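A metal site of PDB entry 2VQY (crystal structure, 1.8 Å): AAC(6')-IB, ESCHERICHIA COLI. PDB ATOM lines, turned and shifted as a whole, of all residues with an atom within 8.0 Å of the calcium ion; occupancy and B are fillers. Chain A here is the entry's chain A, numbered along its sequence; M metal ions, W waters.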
ATOM      1  N   GLN A 193      -9.517  12.763   6.293  1.00  0.00           N
ATOM      2  CA  GLN A 193      -8.610  13.284   5.237  1.00  0.00           C
ATOM      3  C   GLN A 193      -7.902  14.582   5.647  1.00  0.00           C
ATOM      4  O   GLN A 193      -6.709  14.737   5.406  1.00  0.00           O
ATOM      5  CB  GLN A 193      -9.353  13.446   3.919  1.00  0.00           C
ATOM      6  CG  GLN A 193      -8.447  13.872   2.734  1.00  0.00           C
ATOM      7  CD  GLN A 193      -9.181  13.846   1.395  1.00  0.00           C
ATOM      8  OE1 GLN A 193     -10.089  14.662   1.139  1.00  0.00           O
ATOM      9  NE2 GLN A 193      -8.794  12.902   0.521  1.00  0.00           N
ATOM     10  N   ALA A 194      -8.655  15.509   6.253  1.00  0.00           N
ATOM     11  CA  ALA A 194      -8.083  16.747   6.806  1.00  0.00           C
ATOM     12  C   ALA A 194      -6.990  16.502   7.832  1.00  0.00           C
ATOM     13  O   ALA A 194      -5.926  17.113   7.756  1.00  0.00           O
ATOM     14  CB  ALA A 194      -9.202  17.664   7.366  1.00  0.00           C
ATOM     15  N   PHE A 195      -7.235  15.573   8.762  1.00  0.00           N
ATOM     16  CA  PHE A 195      -6.274  15.215   9.796  1.00  0.00           C
ATOM     17  C   PHE A 195      -4.971  14.664   9.171  1.00  0.00           C
ATOM     18  O   PHE A 195      -3.880  15.025   9.608  1.00  0.00           O
ATOM     19  CB  PHE A 195      -6.902  14.152  10.712  1.00  0.00           C
ATOM     20  CG  PHE A 195      -6.006  13.689  11.830  1.00  0.00           C
ATOM     21  CD1 PHE A 195      -5.806  14.482  12.962  1.00  0.00           C
ATOM     22  CD2 PHE A 195      -5.377  12.440  11.759  1.00  0.00           C
ATOM     23  CE1 PHE A 195      -4.964  14.038  14.023  1.00  0.00           C
ATOM     24  CE2 PHE A 195      -4.556  11.966  12.794  1.00  0.00           C
ATOM     25  CZ  PHE A 195      -4.331  12.777  13.940  1.00  0.00           C
ATOM     26  N   GLU A 196      -5.131  13.806   8.151  1.00  0.00           N
ATOM     27  CA  GLU A 196      -3.985  13.200   7.423  1.00  0.00           C
ATOM     28  C   GLU A 196      -3.159  14.303   6.773  1.00  0.00           C
ATOM     29  O   GLU A 196      -1.946  14.354   6.930  1.00  0.00           O
ATOM     30  CB  GLU A 196      -4.469  12.216   6.350  1.00  0.00           C
ATOM     31  CG  GLU A 196      -5.021  10.889   6.895  1.00  0.00           C
ATOM     32  CD  GLU A 196      -5.785  10.098   5.873  1.00  0.00           C
ATOM     33  OE1 GLU A 196      -5.889  10.573   4.716  1.00  0.00           O
ATOM     34  OE2 GLU A 196      -6.315   9.011   6.211  1.00  0.00           O
ATOM     35  N   ARG A 197      -3.859  15.197   6.083  1.00  0.00           N
ATOM     36  CA  ARG A 197      -3.236  16.287   5.328  1.00  0.00           C
ATOM     37  C   ARG A 197      -2.465  17.222   6.207  1.00  0.00           C
ATOM     38  O   ARG A 197      -1.405  17.713   5.804  1.00  0.00           O
ATOM     39  CB  ARG A 197      -4.272  17.050   4.512  1.00  0.00           C
ATOM     40  CG  ARG A 197      -4.693  16.347   3.235  1.00  0.00           C
ATOM     41  CD  ARG A 197      -5.529  17.311   2.403  1.00  0.00           C
ATOM     42  NE  ARG A 197      -6.974  17.176   2.622  1.00  0.00           N
ATOM     43  CZ  ARG A 197      -7.726  17.992   3.368  1.00  0.00           C
ATOM     44  NH1 ARG A 197      -7.196  19.022   4.036  1.00  0.00           N
ATOM     45  NH2 ARG A 197      -9.027  17.757   3.470  1.00  0.00           N
ATOM     46  N   THR A 198      -2.957  17.461   7.426  1.00  0.00           N
ATOM     47  CA  THR A 198      -2.322  18.418   8.320  1.00  0.00           C
ATOM     48  C   THR A 198      -1.288  17.826   9.281  1.00  0.00           C
ATOM     49  O   THR A 198      -0.748  18.545  10.127  1.00  0.00           O
ATOM     50  CB  THR A 198      -3.365  19.227   9.118  1.00  0.00           C
ATOM     51  OG1 THR A 198      -4.108  18.321   9.951  1.00  0.00           O
ATOM     52  CG2 THR A 198      -4.310  19.990   8.180  1.00  0.00           C
ATOM     53  N   ARG A 199      -1.002  16.528   9.158  1.00  0.00           N
ATOM     54  CA  ARG A 199       0.023  15.895  10.017  1.00  0.00           C
ATOM     55  C   ARG A 199       1.432  16.347   9.696  1.00  0.00           C
ATOM     56  O   ARG A 199       2.327  16.287  10.551  1.00  0.00           O
ATOM     57  CB  ARG A 199       0.000  14.366   9.936  1.00  0.00           C
ATOM     58  CG  ARG A 199      -1.173  13.700  10.630  1.00  0.00           C
ATOM     59  CD  ARG A 199      -1.517  14.306  11.968  1.00  0.00           C
ATOM     60  NE  ARG A 199      -2.451  15.428  11.828  1.00  0.00           N
ATOM     61  CZ  ARG A 199      -2.703  16.313  12.785  1.00  0.00           C
ATOM     62  NH1 ARG A 199      -2.094  16.218  13.948  1.00  0.00           N
ATOM     63  NH2 ARG A 199      -3.578  17.289  12.565  1.00  0.00           N
ATOM     64  N   SER A 200       1.637  16.732   8.439  1.00  0.00           N
ATOM     65  CA  SER A 200       2.918  17.304   8.018  1.00  0.00           C
ATOM     66  C   SER A 200       2.746  18.331   6.894  1.00  0.00           C
ATOM     67  O   SER A 200       1.741  18.346   6.167  1.00  0.00           O
ATOM     68  CB  SER A 200       3.918  16.197   7.608  1.00  0.00           C
ATOM     69  OG  SER A 200       3.709  15.804   6.262  1.00  0.00           O
ATOM     70  N   ASP A 201       3.758  19.194   6.782  1.00  0.00           N
ATOM     71  CA  ASP A 201       3.834  20.209   5.734  1.00  0.00           C
ATOM     72  C   ASP A 201       4.273  19.694   4.374  1.00  0.00           C
ATOM     73  O   ASP A 201       4.283  20.456   3.397  1.00  0.00           O
ATOM     74  CB  ASP A 201       4.735  21.361   6.180  1.00  0.00           C
ATOM     75  CG  ASP A 201       4.053  22.275   7.159  1.00  0.00           C
ATOM     76  OD1 ASP A 201       3.050  22.931   6.771  1.00  0.00           O
ATOM     77  OD2 ASP A 201       4.501  22.331   8.337  1.00  0.00           O
ATOM     78  N   ALA A 202       4.660  18.422   4.319  1.00  0.00           N
ATOM     79  CA  ALA A 202       4.873  17.713   3.052  1.00  0.00           C
ATOM     80  C   ALA A 202       3.561  17.466   2.308  1.00  0.00           C
ATOM     81  O   ALA A 202       2.447  17.479   2.873  1.00  0.00           O
ATOM     82  CB  ALA A 202       5.595  16.397   3.314  1.00  0.00           C
ATOM     83  OXT ALA A 202       3.563  17.267   1.077  1.00  0.00           O
HETATM   84 CA    CA M   1       0.377  17.743   4.327  1.00  0.00          CA
HETATM   85  O   HOH W   1      -0.054  20.119   4.503  1.00  0.00           O
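Of the 10 residues printed, 3 come within 4 Å of the calcium ion.
The calcium ion is bound by the backbone carbonyl oxygen of Arg 197, the backbone carbonyl oxygen of Ser 200, water W1 and the chain-end carboxylate of Ala 202.
The side-chain hydroxyl of Ser 200 sits close to the backbone NH of Ala 202.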
